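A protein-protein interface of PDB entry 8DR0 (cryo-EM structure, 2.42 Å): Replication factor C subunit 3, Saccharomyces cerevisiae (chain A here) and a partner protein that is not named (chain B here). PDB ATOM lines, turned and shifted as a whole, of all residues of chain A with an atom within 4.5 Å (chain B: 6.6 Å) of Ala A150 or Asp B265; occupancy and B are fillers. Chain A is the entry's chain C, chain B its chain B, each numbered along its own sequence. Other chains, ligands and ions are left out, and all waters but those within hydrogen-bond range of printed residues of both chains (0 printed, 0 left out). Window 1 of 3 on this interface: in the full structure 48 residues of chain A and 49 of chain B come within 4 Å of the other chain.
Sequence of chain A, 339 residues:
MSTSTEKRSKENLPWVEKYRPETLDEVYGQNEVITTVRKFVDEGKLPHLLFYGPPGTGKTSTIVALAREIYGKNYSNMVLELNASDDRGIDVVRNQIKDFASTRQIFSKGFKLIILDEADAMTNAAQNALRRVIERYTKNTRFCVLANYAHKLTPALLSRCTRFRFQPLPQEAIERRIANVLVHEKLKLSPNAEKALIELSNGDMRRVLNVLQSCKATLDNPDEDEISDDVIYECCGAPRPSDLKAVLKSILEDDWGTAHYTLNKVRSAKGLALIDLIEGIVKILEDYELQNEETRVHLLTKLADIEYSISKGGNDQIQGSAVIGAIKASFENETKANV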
ATOM      1  N   TYR A  52     -32.570 -17.490 -25.333  1.00  0.00           N
ATOM      2  CA  TYR A  52     -31.157 -17.582 -24.991  1.00  0.00           C
ATOM      3  C   TYR A  52     -30.355 -16.755 -25.984  1.00  0.00           C
ATOM      4  O   TYR A  52     -30.493 -16.936 -27.197  1.00  0.00           O
ATOM      5  CB  TYR A  52     -30.690 -19.038 -25.008  1.00  0.00           C
ATOM      6  CG  TYR A  52     -29.191 -19.206 -24.913  1.00  0.00           C
ATOM      7  CD1 TYR A  52     -28.529 -19.036 -23.705  1.00  0.00           C
ATOM      8  CD2 TYR A  52     -28.439 -19.539 -26.031  1.00  0.00           C
ATOM      9  CE1 TYR A  52     -27.162 -19.190 -23.613  1.00  0.00           C
ATOM     10  CE2 TYR A  52     -27.069 -19.694 -25.949  1.00  0.00           C
ATOM     11  CZ  TYR A  52     -26.435 -19.519 -24.738  1.00  0.00           C
ATOM     12  OH  TYR A  52     -25.071 -19.673 -24.651  1.00  0.00           O
ATOM     13  N   ASN A 148     -28.577 -15.492 -20.772  1.00  0.00           N
ATOM     14  CA  ASN A 148     -27.342 -15.362 -21.532  1.00  0.00           C
ATOM     15  C   ASN A 148     -26.448 -16.586 -21.411  1.00  0.00           C
ATOM     16  O   ASN A 148     -25.673 -16.868 -22.330  1.00  0.00           O
ATOM     17  CB  ASN A 148     -26.554 -14.132 -21.064  1.00  0.00           C
ATOM     18  CG  ASN A 148     -27.302 -12.834 -21.290  1.00  0.00           C
ATOM     19  OD1 ASN A 148     -27.630 -12.122 -20.344  1.00  0.00           O
ATOM     20  ND2 ASN A 148     -27.567 -12.516 -22.551  1.00  0.00           N
ATOM     21  N   TYR A 149     -26.543 -17.317 -20.301  1.00  0.00           N
ATOM     22  CA  TYR A 149     -25.715 -18.491 -20.044  1.00  0.00           C
ATOM     23  C   TYR A 149     -26.631 -19.666 -19.733  1.00  0.00           C
ATOM     24  O   TYR A 149     -27.263 -19.702 -18.672  1.00  0.00           O
ATOM     25  CB  TYR A 149     -24.745 -18.233 -18.889  1.00  0.00           C
ATOM     26  CG  TYR A 149     -24.147 -16.846 -18.903  1.00  0.00           C
ATOM     27  CD1 TYR A 149     -23.211 -16.483 -19.861  1.00  0.00           C
ATOM     28  CD2 TYR A 149     -24.523 -15.897 -17.964  1.00  0.00           C
ATOM     29  CE1 TYR A 149     -22.663 -15.217 -19.881  1.00  0.00           C
ATOM     30  CE2 TYR A 149     -23.980 -14.626 -17.974  1.00  0.00           C
ATOM     31  CZ  TYR A 149     -23.050 -14.292 -18.935  1.00  0.00           C
ATOM     32  OH  TYR A 149     -22.506 -13.028 -18.952  1.00  0.00           O
ATOM     33  N   ALA A 150     -26.699 -20.629 -20.653  1.00  0.00           N
ATOM     34  CA  ALA A 150     -27.588 -21.771 -20.485  1.00  0.00           C
ATOM     35  C   ALA A 150     -27.084 -22.768 -19.452  1.00  0.00           C
ATOM     36  O   ALA A 150     -27.882 -23.556 -18.933  1.00  0.00           O
ATOM     37  CB  ALA A 150     -27.786 -22.482 -21.824  1.00  0.00           C
ATOM     38  N   HIS A 151     -25.786 -22.758 -19.139  1.00  0.00           N
ATOM     39  CA  HIS A 151     -25.239 -23.715 -18.185  1.00  0.00           C
ATOM     40  C   HIS A 151     -25.735 -23.483 -16.763  1.00  0.00           C
ATOM     41  O   HIS A 151     -25.552 -24.362 -15.915  1.00  0.00           O
ATOM     42  CB  HIS A 151     -23.710 -23.668 -18.214  1.00  0.00           C
ATOM     43  CG  HIS A 151     -23.119 -22.579 -17.376  1.00  0.00           C
ATOM     44  ND1 HIS A 151     -22.682 -22.787 -16.086  1.00  0.00           N
ATOM     45  CD2 HIS A 151     -22.889 -21.272 -17.645  1.00  0.00           C
ATOM     46  CE1 HIS A 151     -22.210 -21.655 -15.595  1.00  0.00           C
ATOM     47  NE2 HIS A 151     -22.324 -20.720 -16.521  1.00  0.00           N
ATOM     48  N   LYS A 152     -26.351 -22.338 -16.482  1.00  0.00           N
ATOM     49  CA  LYS A 152     -26.912 -22.059 -15.167  1.00  0.00           C
ATOM     50  C   LYS A 152     -28.367 -22.493 -15.038  1.00  0.00           C
ATOM     51  O   LYS A 152     -28.950 -22.334 -13.961  1.00  0.00           O
ATOM     52  CB  LYS A 152     -26.797 -20.563 -14.851  1.00  0.00           C
ATOM     53  CG  LYS A 152     -25.367 -20.061 -14.753  1.00  0.00           C
ATOM     54  CD  LYS A 152     -24.749 -20.410 -13.409  1.00  0.00           C
ATOM     55  CE  LYS A 152     -24.839 -19.247 -12.435  1.00  0.00           C
ATOM     56  NZ  LYS A 152     -23.890 -18.154 -12.786  1.00  0.00           N
ATOM     57  N   LEU A 153     -28.962 -23.034 -16.096  1.00  0.00           N
ATOM     58  CA  LEU A 153     -30.349 -23.478 -16.080  1.00  0.00           C
ATOM     59  C   LEU A 153     -30.394 -24.986 -15.865  1.00  0.00           C
ATOM     60  O   LEU A 153     -29.683 -25.735 -16.542  1.00  0.00           O
ATOM     61  CB  LEU A 153     -31.052 -23.109 -17.387  1.00  0.00           C
ATOM     62  CG  LEU A 153     -31.094 -21.618 -17.735  1.00  0.00           C
ATOM     63  CD1 LEU A 153     -31.844 -21.397 -19.037  1.00  0.00           C
ATOM     64  CD2 LEU A 153     -31.722 -20.806 -16.612  1.00  0.00           C
ATOM     65  N   HIS B 232     -25.577 -28.304 -29.234  1.00  0.00           N
ATOM     66  CA  HIS B 232     -24.229 -27.750 -29.235  1.00  0.00           C
ATOM     67  C   HIS B 232     -23.212 -28.715 -28.624  1.00  0.00           C
ATOM     68  O   HIS B 232     -22.024 -28.625 -28.959  1.00  0.00           O
ATOM     69  CB  HIS B 232     -24.202 -26.397 -28.514  1.00  0.00           C
ATOM     70  CG  HIS B 232     -24.251 -26.492 -27.022  1.00  0.00           C
ATOM     71  ND1 HIS B 232     -25.433 -26.464 -26.313  1.00  0.00           N
ATOM     72  CD2 HIS B 232     -23.264 -26.592 -26.101  1.00  0.00           C
ATOM     73  CE1 HIS B 232     -25.172 -26.556 -25.021  1.00  0.00           C
ATOM     74  NE2 HIS B 232     -23.862 -26.635 -24.866  1.00  0.00           N
ATOM     75  N   VAL B 236     -19.449 -29.326 -30.095  1.00  0.00           N
ATOM     76  CA  VAL B 236     -18.236 -29.274 -29.286  1.00  0.00           C
ATOM     77  C   VAL B 236     -17.444 -30.567 -29.431  1.00  0.00           C
ATOM     78  O   VAL B 236     -16.210 -30.553 -29.513  1.00  0.00           O
ATOM     79  CB  VAL B 236     -18.593 -28.989 -27.815  1.00  0.00           C
ATOM     80  CG1 VAL B 236     -17.424 -29.320 -26.902  1.00  0.00           C
ATOM     81  CG2 VAL B 236     -19.016 -27.538 -27.645  1.00  0.00           C
ATOM     82  N   GLY B 260     -23.801 -17.001 -31.132  1.00  0.00           N
ATOM     83  CA  GLY B 260     -24.225 -16.382 -29.895  1.00  0.00           C
ATOM     84  C   GLY B 260     -24.021 -17.209 -28.647  1.00  0.00           C
ATOM     85  O   GLY B 260     -24.613 -16.884 -27.611  1.00  0.00           O
ATOM     86  N   TYR B 261     -23.209 -18.260 -28.704  1.00  0.00           N
ATOM     87  CA  TYR B 261     -22.932 -19.066 -27.523  1.00  0.00           C
ATOM     88  C   TYR B 261     -21.842 -18.404 -26.690  1.00  0.00           C
ATOM     89  O   TYR B 261     -20.806 -17.991 -27.220  1.00  0.00           O
ATOM     90  CB  TYR B 261     -22.510 -20.479 -27.925  1.00  0.00           C
ATOM     91  CG  TYR B 261     -23.652 -21.334 -28.415  1.00  0.00           C
ATOM     92  CD1 TYR B 261     -24.474 -22.008 -27.523  1.00  0.00           C
ATOM     93  CD2 TYR B 261     -23.911 -21.470 -29.773  1.00  0.00           C
ATOM     94  CE1 TYR B 261     -25.521 -22.791 -27.966  1.00  0.00           C
ATOM     95  CE2 TYR B 261     -24.955 -22.251 -30.226  1.00  0.00           C
ATOM     96  CZ  TYR B 261     -25.758 -22.909 -29.318  1.00  0.00           C
ATOM     97  OH  TYR B 261     -26.800 -23.688 -29.764  1.00  0.00           O
ATOM     98  N   SER B 262     -22.081 -18.299 -25.386  1.00  0.00           N
ATOM     99  CA  SER B 262     -21.124 -17.656 -24.500  1.00  0.00           C
ATOM    100  C   SER B 262     -19.899 -18.544 -24.295  1.00  0.00           C
ATOM    101  O   SER B 262     -19.949 -19.769 -24.438  1.00  0.00           O
ATOM    102  CB  SER B 262     -21.772 -17.336 -23.154  1.00  0.00           C
ATOM    103  OG  SER B 262     -22.266 -18.508 -22.532  1.00  0.00           O
ATOM    104  N   SER B 263     -18.781 -17.901 -23.951  1.00  0.00           N
ATOM    105  CA  SER B 263     -17.542 -18.639 -23.731  1.00  0.00           C
ATOM    106  C   SER B 263     -17.666 -19.585 -22.544  1.00  0.00           C
ATOM    107  O   SER B 263     -17.116 -20.692 -22.563  1.00  0.00           O
ATOM    108  CB  SER B 263     -16.382 -17.664 -23.525  1.00  0.00           C
ATOM    109  OG  SER B 263     -16.639 -16.785 -22.445  1.00  0.00           O
ATOM    110  N   ILE B 264     -18.377 -19.166 -21.494  1.00  0.00           N
ATOM    111  CA  ILE B 264     -18.542 -20.024 -20.323  1.00  0.00           C
ATOM    112  C   ILE B 264     -19.301 -21.292 -20.697  1.00  0.00           C
ATOM    113  O   ILE B 264     -18.927 -22.401 -20.294  1.00  0.00           O
ATOM    114  CB  ILE B 264     -19.240 -19.247 -19.189  1.00  0.00           C
ATOM    115  CG1 ILE B 264     -19.210 -20.047 -17.883  1.00  0.00           C
ATOM    116  CG2 ILE B 264     -20.677 -18.908 -19.562  1.00  0.00           C
ATOM    117  CD1 ILE B 264     -17.831 -20.173 -17.274  1.00  0.00           C
ATOM    118  N   ASP B 265     -20.373 -21.153 -21.482  1.00  0.00           N
ATOM    119  CA  ASP B 265     -21.115 -22.327 -21.926  1.00  0.00           C
ATOM    120  C   ASP B 265     -20.233 -23.243 -22.762  1.00  0.00           C
ATOM    121  O   ASP B 265     -20.257 -24.467 -22.593  1.00  0.00           O
ATOM    122  CB  ASP B 265     -22.347 -21.901 -22.727  1.00  0.00           C
ATOM    123  CG  ASP B 265     -23.407 -21.241 -21.866  1.00  0.00           C
ATOM    124  OD1 ASP B 265     -23.550 -21.631 -20.688  1.00  0.00           O
ATOM    125  OD2 ASP B 265     -24.103 -20.337 -22.371  1.00  0.00           O
ATOM    126  N   ILE B 266     -19.441 -22.664 -23.667  1.00  0.00           N
ATOM    127  CA  ILE B 266     -18.584 -23.470 -24.529  1.00  0.00           C
ATOM    128  C   ILE B 266     -17.570 -24.244 -23.697  1.00  0.00           C
ATOM    129  O   ILE B 266     -17.343 -25.436 -23.923  1.00  0.00           O
ATOM    130  CB  ILE B 266     -17.891 -22.582 -25.579  1.00  0.00           C
ATOM    131  CG1 ILE B 266     -18.925 -21.993 -26.541  1.00  0.00           C
ATOM    132  CG2 ILE B 266     -16.848 -23.383 -26.344  1.00  0.00           C
ATOM    133  CD1 ILE B 266     -18.436 -20.772 -27.292  1.00  0.00           C
ATOM    134  N   VAL B 267     -16.946 -23.584 -22.719  1.00  0.00           N
ATOM    135  CA  VAL B 267     -15.909 -24.246 -21.934  1.00  0.00           C
ATOM    136  C   VAL B 267     -16.516 -25.330 -21.048  1.00  0.00           C
ATOM    137  O   VAL B 267     -15.940 -26.413 -20.890  1.00  0.00           O
ATOM    138  CB  VAL B 267     -15.106 -23.209 -21.122  1.00  0.00           C
ATOM    139  CG1 VAL B 267     -15.735 -22.950 -19.758  1.00  0.00           C
ATOM    140  CG2 VAL B 267     -13.663 -23.659 -20.971  1.00  0.00           C
ATOM    141  N   THR B 268     -17.693 -25.070 -20.468  1.00  0.00           N
ATOM    142  CA  THR B 268     -18.345 -26.091 -19.651  1.00  0.00           C
ATOM    143  C   THR B 268     -18.732 -27.304 -20.493  1.00  0.00           C
ATOM    144  O   THR B 268     -18.529 -28.455 -20.080  1.00  0.00           O
ATOM    145  CB  THR B 268     -19.572 -25.496 -18.959  1.00  0.00           C
ATOM    146  OG1 THR B 268     -19.155 -24.692 -17.849  1.00  0.00           O
ATOM    147  CG2 THR B 268     -20.501 -26.594 -18.459  1.00  0.00           C
ATOM    148  N   THR B 269     -19.288 -27.063 -21.684  1.00  0.00           N
ATOM    149  CA  THR B 269     -19.644 -28.165 -22.568  1.00  0.00           C
ATOM    150  C   THR B 269     -18.407 -28.941 -22.995  1.00  0.00           C
ATOM    151  O   THR B 269     -18.441 -30.173 -23.094  1.00  0.00           O
ATOM    152  CB  THR B 269     -20.391 -27.635 -23.792  1.00  0.00           C
ATOM    153  OG1 THR B 269     -21.606 -26.999 -23.376  1.00  0.00           O
ATOM    154  CG2 THR B 269     -20.721 -28.768 -24.753  1.00  0.00           C
ATOM    155  N   SER B 270     -17.306 -28.237 -23.266  1.00  0.00           N
ATOM    156  CA  SER B 270     -16.063 -28.914 -23.616  1.00  0.00           C
ATOM    157  C   SER B 270     -15.592 -29.804 -22.477  1.00  0.00           C
ATOM    158  O   SER B 270     -15.169 -30.942 -22.703  1.00  0.00           O
ATOM    159  CB  SER B 270     -14.989 -27.886 -23.971  1.00  0.00           C
ATOM    160  OG  SER B 270     -15.335 -27.166 -25.142  1.00  0.00           O
ATOM    161  N   ARG B 272     -17.434 -31.239 -20.130  1.00  0.00           N
ATOM    162  CA  ARG B 272     -18.304 -32.410 -20.026  1.00  0.00           C
ATOM    163  C   ARG B 272     -18.027 -33.411 -21.146  1.00  0.00           C
ATOM    164  O   ARG B 272     -17.907 -34.620 -20.899  1.00  0.00           O
ATOM    165  CB  ARG B 272     -19.771 -31.979 -20.045  1.00  0.00           C
ATOM    166  CG  ARG B 272     -20.343 -31.696 -18.665  1.00  0.00           C
ATOM    167  CD  ARG B 272     -21.832 -31.390 -18.722  1.00  0.00           C
ATOM    168  NE  ARG B 272     -22.125 -30.204 -19.520  1.00  0.00           N
ATOM    169  CZ  ARG B 272     -22.738 -30.209 -20.698  1.00  0.00           C
ATOM    170  NH1 ARG B 272     -23.130 -31.335 -21.274  1.00  0.00           N
ATOM    171  NH2 ARG B 272     -22.962 -29.053 -21.315  1.00  0.00           N
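Of the printed residues of chain B, Asn A148 touches Ser B262 (3.8 Å) and Asp B265 (3.8 Å). Ala A150 touches one residue of chain B. Of the printed residues of chain B, His A151 touches Ile B264 and Asp B265. Ser B263 touches none of the printed residues of chain A. Asp B265 touches just these residues of chain A: Tyr A52, Asn A148, Tyr A149, Ala A150 and His A151. The nearest residue of chain B that does not touch Ala A150 is Ser B262 (5.3 Å). The nearest printed residue of chain A that does not touch Asp B265 is Lys A152 (5.1 Å).
OH of Tyr A52 touches CA of Tyr B261, at 3.6 Å. O of Asn A148 touches OG of Ser B262, 3.8 Å away. Asn A148 touches Asp B265 (O to OD2, 3.8 Å). CD1 of Tyr A149 touches OG of Ser B262, 3.5 Å away. Ile B264 touches Tyr A149 (CG2 to CD1, 3.5 Å). Tyr A149 touches Asp B265 (CA to OD2, 3.4 Å). His A151 touches Ile B264.
N of Ser B262 sits at hydrogen-bond distance from OH of Tyr A52. The side-chain carboxylate (OD2) of Asp B265 lies within hydrogen-bond range of the backbone NH (N) of Ala A150. The backbone NH of His A151 is in hydrogen-bond range of the side-chain carboxylate of Asp B265 (2.9 Å). OD2 of Asp B265 lies within hydrogen-bond range of OH of Tyr A52.
The side-chain carboxylate (OD2) of Asp B265 lies within hydrogen-bond range of the side-chain hydroxyl (OG) of Ser B262 (2.6 Å). The backbone carbonyl oxygen (O) of Ile B264 lies within hydrogen-bond range of the side-chain hydroxyl (OG1) of Thr B268 (3.4 Å). The side-chain hydroxyl (OG1) of Thr B269 lies within hydrogen-bond range of the backbone carbonyl oxygen (O) of Asp B265 (3.0 Å).
Printed residues of chain B that touch a printed residue of chain A: Tyr B261, Ser B262, Ile B264 and Asp B265. Hydrophobic or aromatic side chains of chain B that line the printed part of chain A: Tyr B261 and Ile B264. Printed residues of chain A that touch a printed residue of chain B: Tyr A52, Asn A148, Tyr A149, Ala A150 and His A151. Hydrophobic or aromatic side chains of chain A that line the printed part of chain B: Tyr A52, Tyr A149 and His A151. Along chain A the printed residues that touch a printed residue of chain B span positions 52 to 151. Among the printed residues, 11 pairs touch across the chains.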
